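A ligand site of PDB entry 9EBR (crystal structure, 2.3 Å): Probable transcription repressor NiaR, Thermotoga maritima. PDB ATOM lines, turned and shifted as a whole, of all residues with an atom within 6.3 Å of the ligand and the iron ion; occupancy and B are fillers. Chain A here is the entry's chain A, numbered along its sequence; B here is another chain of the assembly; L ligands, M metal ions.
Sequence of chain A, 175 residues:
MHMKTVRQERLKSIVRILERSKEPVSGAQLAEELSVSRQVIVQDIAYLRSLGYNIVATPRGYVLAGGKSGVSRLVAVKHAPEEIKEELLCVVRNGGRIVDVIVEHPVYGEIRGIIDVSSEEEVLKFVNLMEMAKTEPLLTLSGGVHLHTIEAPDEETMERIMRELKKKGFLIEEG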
ATOM      1  N   VAL A  77       5.364 -26.002   0.495  1.00  0.00           N
ATOM      2  CA  VAL A  77       5.922 -26.482  -0.763  1.00  0.00           C
ATOM      3  C   VAL A  77       7.407 -26.763  -0.572  1.00  0.00           C
ATOM      4  O   VAL A  77       7.999 -26.434   0.445  1.00  0.00           O
ATOM      5  CB  VAL A  77       5.715 -25.476  -1.916  1.00  0.00           C
ATOM      6  CG1 VAL A  77       4.229 -25.194  -2.106  1.00  0.00           C
ATOM      7  CG2 VAL A  77       6.525 -24.205  -1.647  1.00  0.00           C
ATOM      8  N   HIS A  79      10.904 -26.967  -3.453  1.00  0.00           N
ATOM      9  CA  HIS A  79      11.459 -27.025  -4.799  1.00  0.00           C
ATOM     10  C   HIS A  79      12.805 -26.324  -4.785  1.00  0.00           C
ATOM     11  O   HIS A  79      13.159 -25.611  -3.834  1.00  0.00           O
ATOM     12  CB  HIS A  79      10.523 -26.376  -5.798  1.00  0.00           C
ATOM     13  CG  HIS A  79      10.242 -24.951  -5.497  1.00  0.00           C
ATOM     14  ND1 HIS A  79      11.203 -23.971  -5.587  1.00  0.00           N
ATOM     15  CD2 HIS A  79       9.106 -24.341  -5.082  1.00  0.00           C
ATOM     16  CE1 HIS A  79      10.680 -22.812  -5.253  1.00  0.00           C
ATOM     17  NE2 HIS A  79       9.407 -23.008  -4.941  1.00  0.00           N
ATOM     18  N   GLU A  83      13.342 -23.770  -9.797  1.00  0.00           N
ATOM     19  CA  GLU A  83      11.927 -24.016 -10.026  1.00  0.00           C
ATOM     20  C   GLU A  83      11.060 -22.842  -9.573  1.00  0.00           C
ATOM     21  O   GLU A  83       9.824 -23.005  -9.465  1.00  0.00           O
ATOM     22  CB  GLU A  83      11.508 -25.299  -9.310  1.00  0.00           C
ATOM     23  CG  GLU A  83      12.629 -26.351  -9.249  1.00  0.00           C
ATOM     24  CD  GLU A  83      12.121 -27.778  -9.090  1.00  0.00           C
ATOM     25  OE1 GLU A  83      11.771 -28.410 -10.093  1.00  0.00           O
ATOM     26  OE2 GLU A  83      12.094 -28.288  -7.942  1.00  0.00           O
ATOM     27  N   ILE A  84      11.655 -21.675  -9.291  1.00  0.00           N
ATOM     28  CA  ILE A  84      10.854 -20.570  -8.788  1.00  0.00           C
ATOM     29  C   ILE A  84       9.906 -20.059  -9.874  1.00  0.00           C
ATOM     30  O   ILE A  84       8.726 -19.785  -9.596  1.00  0.00           O
ATOM     31  CB  ILE A  84      11.753 -19.438  -8.242  1.00  0.00           C
ATOM     32  CG1 ILE A  84      12.379 -19.867  -6.915  1.00  0.00           C
ATOM     33  CG2 ILE A  84      10.965 -18.132  -8.061  1.00  0.00           C
ATOM     34  CD1 ILE A  84      13.427 -18.938  -6.392  1.00  0.00           C
ATOM     35  N   GLU A  87       6.773 -22.273 -10.458  1.00  0.00           N
ATOM     36  CA  GLU A  87       5.831 -22.151  -9.354  1.00  0.00           C
ATOM     37  C   GLU A  87       5.083 -20.827  -9.409  1.00  0.00           C
ATOM     38  O   GLU A  87       3.848 -20.801  -9.345  1.00  0.00           O
ATOM     39  CB  GLU A  87       6.565 -22.310  -8.028  1.00  0.00           C
ATOM     40  CG  GLU A  87       5.656 -22.163  -6.820  1.00  0.00           C
ATOM     41  CD  GLU A  87       6.423 -21.936  -5.512  1.00  0.00           C
ATOM     42  OE1 GLU A  87       7.055 -20.894  -5.398  1.00  0.00           O
ATOM     43  OE2 GLU A  87       6.402 -22.800  -4.598  1.00  0.00           O
ATOM     44  N   LEU A  88       5.803 -19.716  -9.534  1.00  0.00           N
ATOM     45  CA  LEU A  88       5.144 -18.416  -9.560  1.00  0.00           C
ATOM     46  C   LEU A  88       4.191 -18.300 -10.742  1.00  0.00           C
ATOM     47  O   LEU A  88       3.009 -17.949 -10.570  1.00  0.00           O
ATOM     48  CB  LEU A  88       6.188 -17.286  -9.568  1.00  0.00           C
ATOM     49  CG  LEU A  88       7.088 -17.136  -8.324  1.00  0.00           C
ATOM     50  CD1 LEU A  88       7.986 -15.886  -8.386  1.00  0.00           C
ATOM     51  CD2 LEU A  88       6.267 -17.118  -7.039  1.00  0.00           C
ATOM     52  N   ILE A  98       1.239 -14.253  -5.244  1.00  0.00           N
ATOM     53  CA  ILE A  98       2.200 -14.798  -4.288  1.00  0.00           C
ATOM     54  C   ILE A  98       2.611 -13.653  -3.376  1.00  0.00           C
ATOM     55  O   ILE A  98       3.408 -12.815  -3.767  1.00  0.00           O
ATOM     56  CB  ILE A  98       3.420 -15.435  -4.947  1.00  0.00           C
ATOM     57  CG1 ILE A  98       3.005 -16.442  -6.006  1.00  0.00           C
ATOM     58  CG2 ILE A  98       4.308 -16.098  -3.842  1.00  0.00           C
ATOM     59  CD1 ILE A  98       2.640 -15.798  -7.342  1.00  0.00           C
ATOM     60  N   VAL A 101       7.275 -15.362   0.979  1.00  0.00           N
ATOM     61  CA  VAL A 101       7.867 -16.655   1.241  1.00  0.00           C
ATOM     62  C   VAL A 101       8.308 -16.651   2.687  1.00  0.00           C
ATOM     63  O   VAL A 101       8.842 -15.652   3.175  1.00  0.00           O
ATOM     64  CB  VAL A 101       9.074 -16.955   0.346  1.00  0.00           C
ATOM     65  CG1 VAL A 101      10.094 -15.856   0.465  1.00  0.00           C
ATOM     66  CG2 VAL A 101       9.677 -18.284   0.771  1.00  0.00           C
ATOM     67  N   VAL A 103      10.423 -19.077   5.434  1.00  0.00           N
ATOM     68  CA  VAL A 103      11.220 -20.241   5.768  1.00  0.00           C
ATOM     69  C   VAL A 103      11.264 -20.404   7.279  1.00  0.00           C
ATOM     70  O   VAL A 103      11.336 -19.423   8.023  1.00  0.00           O
ATOM     71  CB  VAL A 103      12.627 -20.074   5.172  1.00  0.00           C
ATOM     72  CG1 VAL A 103      13.584 -21.035   5.840  1.00  0.00           C
ATOM     73  CG2 VAL A 103      12.546 -20.340   3.688  1.00  0.00           C
ATOM     74  N   ILE A 115       7.204 -10.887  -1.630  1.00  0.00           N
ATOM     75  CA  ILE A 115       7.178 -11.271  -3.037  1.00  0.00           C
ATOM     76  C   ILE A 115       6.170 -10.404  -3.791  1.00  0.00           C
ATOM     77  O   ILE A 115       6.540  -9.716  -4.747  1.00  0.00           O
ATOM     78  CB  ILE A 115       6.894 -12.767  -3.190  1.00  0.00           C
ATOM     79  CG1 ILE A 115       8.010 -13.574  -2.512  1.00  0.00           C
ATOM     80  CG2 ILE A 115       6.774 -13.177  -4.630  1.00  0.00           C
ATOM     81  CD1 ILE A 115       7.880 -15.102  -2.700  1.00  0.00           C
ATOM     82  N   PHE A 126      10.940 -10.592 -11.194  1.00  0.00           N
ATOM     83  CA  PHE A 126      11.396 -11.222  -9.947  1.00  0.00           C
ATOM     84  C   PHE A 126      12.427 -12.314 -10.222  1.00  0.00           C
ATOM     85  O   PHE A 126      13.442 -12.403  -9.521  1.00  0.00           O
ATOM     86  CB  PHE A 126      10.196 -11.771  -9.183  1.00  0.00           C
ATOM     87  CG  PHE A 126      10.535 -12.420  -7.863  1.00  0.00           C
ATOM     88  CD1 PHE A 126      10.956 -13.734  -7.812  1.00  0.00           C
ATOM     89  CD2 PHE A 126      10.435 -11.705  -6.693  1.00  0.00           C
ATOM     90  CE1 PHE A 126      11.293 -14.306  -6.598  1.00  0.00           C
ATOM     91  CE2 PHE A 126      10.756 -12.302  -5.472  1.00  0.00           C
ATOM     92  CZ  PHE A 126      11.172 -13.598  -5.429  1.00  0.00           C
ATOM     93  N   MET A 130      16.436 -12.465  -8.982  1.00  0.00           N
ATOM     94  CA  MET A 130      16.921 -13.597  -8.202  1.00  0.00           C
ATOM     95  C   MET A 130      18.013 -14.353  -8.945  1.00  0.00           C
ATOM     96  O   MET A 130      18.971 -14.849  -8.324  1.00  0.00           O
ATOM     97  CB  MET A 130      15.738 -14.522  -7.881  1.00  0.00           C
ATOM     98  CG  MET A 130      16.005 -15.535  -6.785  1.00  0.00           C
ATOM     99  SD  MET A 130      16.202 -14.764  -5.154  1.00  0.00           S
ATOM    100  CE  MET A 130      14.495 -14.688  -4.535  1.00  0.00           C
ATOM    101  N   GLU A 136      20.444 -15.233  -3.484  1.00  0.00           N
ATOM    102  CA  GLU A 136      19.983 -16.594  -3.296  1.00  0.00           C
ATOM    103  C   GLU A 136      18.615 -16.617  -2.645  1.00  0.00           C
ATOM    104  O   GLU A 136      18.348 -15.825  -1.730  1.00  0.00           O
ATOM    105  CB  GLU A 136      20.964 -17.363  -2.410  1.00  0.00           C
ATOM    106  CG  GLU A 136      22.367 -17.219  -2.905  1.00  0.00           C
ATOM    107  CD  GLU A 136      22.564 -17.960  -4.200  1.00  0.00           C
ATOM    108  OE1 GLU A 136      21.927 -19.016  -4.363  1.00  0.00           O
ATOM    109  OE2 GLU A 136      23.342 -17.464  -5.055  1.00  0.00           O
ATOM    110  N   PRO A 137      17.719 -17.511  -3.060  1.00  0.00           N
ATOM    111  CA  PRO A 137      16.365 -17.531  -2.487  1.00  0.00           C
ATOM    112  C   PRO A 137      16.386 -18.053  -1.056  1.00  0.00           C
ATOM    113  O   PRO A 137      17.288 -18.782  -0.641  1.00  0.00           O
ATOM    114  CB  PRO A 137      15.592 -18.471  -3.410  1.00  0.00           C
ATOM    115  CG  PRO A 137      16.514 -18.721  -4.597  1.00  0.00           C
ATOM    116  CD  PRO A 137      17.896 -18.525  -4.108  1.00  0.00           C
ATOM    117  N   LEU A 138      15.352 -17.685  -0.294  1.00  0.00           N
ATOM    118  CA  LEU A 138      15.305 -18.108   1.104  1.00  0.00           C
ATOM    119  C   LEU A 138      15.321 -19.631   1.236  1.00  0.00           C
ATOM    120  O   LEU A 138      15.940 -20.159   2.163  1.00  0.00           O
ATOM    121  CB  LEU A 138      14.081 -17.500   1.804  1.00  0.00           C
ATOM    122  CG  LEU A 138      14.119 -15.976   1.881  1.00  0.00           C
ATOM    123  CD1 LEU A 138      13.013 -15.358   2.733  1.00  0.00           C
ATOM    124  CD2 LEU A 138      15.481 -15.541   2.400  1.00  0.00           C
ATOM    125  N   LEU A 139      14.696 -20.362   0.303  1.00  0.00           N
ATOM    126  CA  LEU A 139      14.642 -21.822   0.422  1.00  0.00           C
ATOM    127  C   LEU A 139      16.037 -22.446   0.544  1.00  0.00           C
ATOM    128  O   LEU A 139      16.130 -23.623   0.932  1.00  0.00           O
ATOM    129  CB  LEU A 139      13.892 -22.431  -0.774  1.00  0.00           C
ATOM    130  CG  LEU A 139      14.420 -22.155  -2.179  1.00  0.00           C
ATOM    131  CD1 LEU A 139      15.449 -23.185  -2.593  1.00  0.00           C
ATOM    132  CD2 LEU A 139      13.295 -22.055  -3.216  1.00  0.00           C
ATOM    133  N   THR A 140      17.103 -21.696   0.258  1.00  0.00           N
ATOM    134  CA  THR A 140      18.444 -22.263   0.392  1.00  0.00           C
ATOM    135  C   THR A 140      18.871 -22.367   1.842  1.00  0.00           C
ATOM    136  O   THR A 140      19.789 -23.139   2.155  1.00  0.00           O
ATOM    137  CB  THR A 140      19.450 -21.435  -0.421  1.00  0.00           C
ATOM    138  OG1 THR A 140      19.337 -20.055  -0.069  1.00  0.00           O
ATOM    139  CG2 THR A 140      19.182 -21.590  -1.899  1.00  0.00           C
ATOM    140  N   HIS A 146       9.634 -24.749   2.202  1.00  0.00           N
ATOM    141  CA  HIS A 146       9.292 -23.408   2.641  1.00  0.00           C
ATOM    142  C   HIS A 146       7.800 -23.215   2.466  1.00  0.00           C
ATOM    143  O   HIS A 146       7.112 -24.061   1.899  1.00  0.00           O
ATOM    144  CB  HIS A 146      10.052 -22.358   1.842  1.00  0.00           C
ATOM    145  CG  HIS A 146       9.762 -22.385   0.381  1.00  0.00           C
ATOM    146  ND1 HIS A 146      10.241 -23.388  -0.451  1.00  0.00           N
ATOM    147  CD2 HIS A 146       9.055 -21.549  -0.419  1.00  0.00           C
ATOM    148  CE1 HIS A 146       9.847 -23.148  -1.687  1.00  0.00           C
ATOM    149  NE2 HIS A 146       9.135 -22.032  -1.694  1.00  0.00           N
ATOM    150  N   LEU A 147       7.325 -22.037   2.879  1.00  0.00           N
ATOM    151  CA  LEU A 147       5.919 -21.702   2.816  1.00  0.00           C
ATOM    152  C   LEU A 147       5.717 -20.519   1.884  1.00  0.00           C
ATOM    153  O   LEU A 147       6.618 -19.697   1.678  1.00  0.00           O
ATOM    154  CB  LEU A 147       5.364 -21.367   4.208  1.00  0.00           C
ATOM    155  CG  LEU A 147       5.524 -22.439   5.282  1.00  0.00           C
ATOM    156  CD1 LEU A 147       5.188 -21.881   6.661  1.00  0.00           C
ATOM    157  CD2 LEU A 147       4.683 -23.676   5.010  1.00  0.00           C
ATOM    158  N   HIS A 148       4.518 -20.426   1.329  1.00  0.00           N
ATOM    159  CA  HIS A 148       4.087 -19.225   0.631  1.00  0.00           C
ATOM    160  C   HIS A 148       2.727 -18.814   1.161  1.00  0.00           C
ATOM    161  O   HIS A 148       1.904 -19.673   1.503  1.00  0.00           O
ATOM    162  CB  HIS A 148       4.011 -19.462  -0.869  1.00  0.00           C
ATOM    163  CG  HIS A 148       5.334 -19.446  -1.548  1.00  0.00           C
ATOM    164  ND1 HIS A 148       6.169 -18.354  -1.530  1.00  0.00           N
ATOM    165  CD2 HIS A 148       5.962 -20.390  -2.293  1.00  0.00           C
ATOM    166  CE1 HIS A 148       7.256 -18.622  -2.217  1.00  0.00           C
ATOM    167  NE2 HIS A 148       7.142 -19.837  -2.714  1.00  0.00           N
ATOM    168  N   HIS B 105      19.320  -8.102   1.506  1.00  0.00           N
ATOM    169  CA  HIS B 105      19.078  -9.004   0.393  1.00  0.00           C
ATOM    170  C   HIS B 105      18.651  -8.219  -0.845  1.00  0.00           C
ATOM    171  O   HIS B 105      17.701  -7.425  -0.766  1.00  0.00           O
ATOM    172  CB  HIS B 105      18.016 -10.034   0.772  1.00  0.00           C
ATOM    173  CG  HIS B 105      17.821 -11.126  -0.240  1.00  0.00           C
ATOM    174  ND1 HIS B 105      17.209 -10.898  -1.462  1.00  0.00           N
ATOM    175  CD2 HIS B 105      18.158 -12.439  -0.222  1.00  0.00           C
ATOM    176  CE1 HIS B 105      17.168 -12.033  -2.137  1.00  0.00           C
ATOM    177  NE2 HIS B 105      17.746 -12.973  -1.413  1.00  0.00           N
ATOM    178  N   TYR B 108      14.826  -9.189  -1.476  1.00  0.00           N
ATOM    179  CA  TYR B 108      13.934  -9.033  -0.334  1.00  0.00           C
ATOM    180  C   TYR B 108      14.259  -7.835   0.557  1.00  0.00           C
ATOM    181  O   TYR B 108      13.470  -7.495   1.444  1.00  0.00           O
ATOM    182  CB  TYR B 108      13.973 -10.299   0.493  1.00  0.00           C
ATOM    183  CG  TYR B 108      13.442 -11.485  -0.245  1.00  0.00           C
ATOM    184  CD1 TYR B 108      12.231 -11.394  -0.968  1.00  0.00           C
ATOM    185  CD2 TYR B 108      14.113 -12.684  -0.235  1.00  0.00           C
ATOM    186  CE1 TYR B 108      11.736 -12.496  -1.628  1.00  0.00           C
ATOM    187  CE2 TYR B 108      13.612 -13.783  -0.911  1.00  0.00           C
ATOM    188  CZ  TYR B 108      12.446 -13.671  -1.597  1.00  0.00           C
ATOM    189  OH  TYR B 108      11.983 -14.769  -2.273  1.00  0.00           O
HETATM  190  N1  LIG L   1       9.737 -19.412  -3.941  1.00  0.00           N
HETATM  191  C1  LIG L   1      10.764 -19.379  -3.064  1.00  0.00           C
HETATM  192  C2  LIG L   1      11.542 -18.238  -2.972  1.00  0.00           C
HETATM  193  C3  LIG L   1      11.239 -17.178  -3.771  1.00  0.00           C
HETATM  194  C4  LIG L   1      10.187 -17.232  -4.648  1.00  0.00           C
HETATM  195  C5  LIG L   1       9.412 -18.382  -4.736  1.00  0.00           C
HETATM  196  C6  LIG L   1      12.714 -18.137  -1.987  1.00  0.00           C
HETATM  197  O1  LIG L   1      13.237 -19.153  -1.455  1.00  0.00           O
HETATM  198  O2  LIG L   1      13.152 -16.998  -1.671  1.00  0.00           O
HETATM  199 FE    FE M   1       8.401 -21.393  -3.773  1.00  0.00          FE
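The side-chain hydroxyl (OH) of Tyr 108 of chain B is in hydrogen-bond range of an oxygen (O2) of the ligand (2.6 Å). An oxygen (O1) of the ligand sits at hydrogen-bond distance from the backbone NH (N) of Leu 139 (2.6 Å). The backbone NH (N) of Leu 138 sits at hydrogen-bond distance from an oxygen (O2) of the ligand.
N of His 146 is in hydrogen-bond range of O of Val 77, at 2.9 Å. The side-chain hydroxyl (OG1) of Thr 140 lies within hydrogen-bond range of the backbone carbonyl oxygen (O) of Pro 137 (2.5 Å). ND1 of His 105 of chain B lies within hydrogen-bond range of N of Tyr 108 of chain B.
Ile 84 touches the ligand. CG1 of Val 101 touches O2 of the ligand, 3.9 Å away. CD1 of Ile 115 touches C4 of the ligand, at 3.7 Å. CE1 of Phe 126 touches C4 of the ligand, at 3.7 Å. Met 130 touches the ligand. Pro 137 touches the ligand (CB to O1, 3.1 Å). 13 residues have an atom within 4 Å of the ligand: His 79, Ile 84, Glu 87, Val 101, Ile 115, Phe 126, Met 130, Pro 137, Leu 138, Leu 139, His 146, His 148 and Tyr 108 of chain B. The nearest printed residue that does not touch the ligand is Leu 88 (4.1 Å).
CG2 of Val 77 touches the iron ion, at 3.99 Å. Five residues have an atom within 4 Å of the iron ion: Val 77, His 79, Glu 87, His 146 and His 148. The nearest printed residue that does not touch the iron ion is Leu 139 (5.0 Å).
OE1 of Glu 87 is bound to the iron ion. The iron ion is bound by a ring nitrogen (NE2) of His 79. NE2 of His 148 is bound to the iron ion. The iron ion is bound by a ring nitrogen (NE2) of His 146 (2.3 Å). A nitrogen (N1) of the ligand binds the iron ion. The side-chain carboxylate (OE2) of Glu 87 binds the iron ion (2.6 Å). The iron ion has six donor atoms within binding distance.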
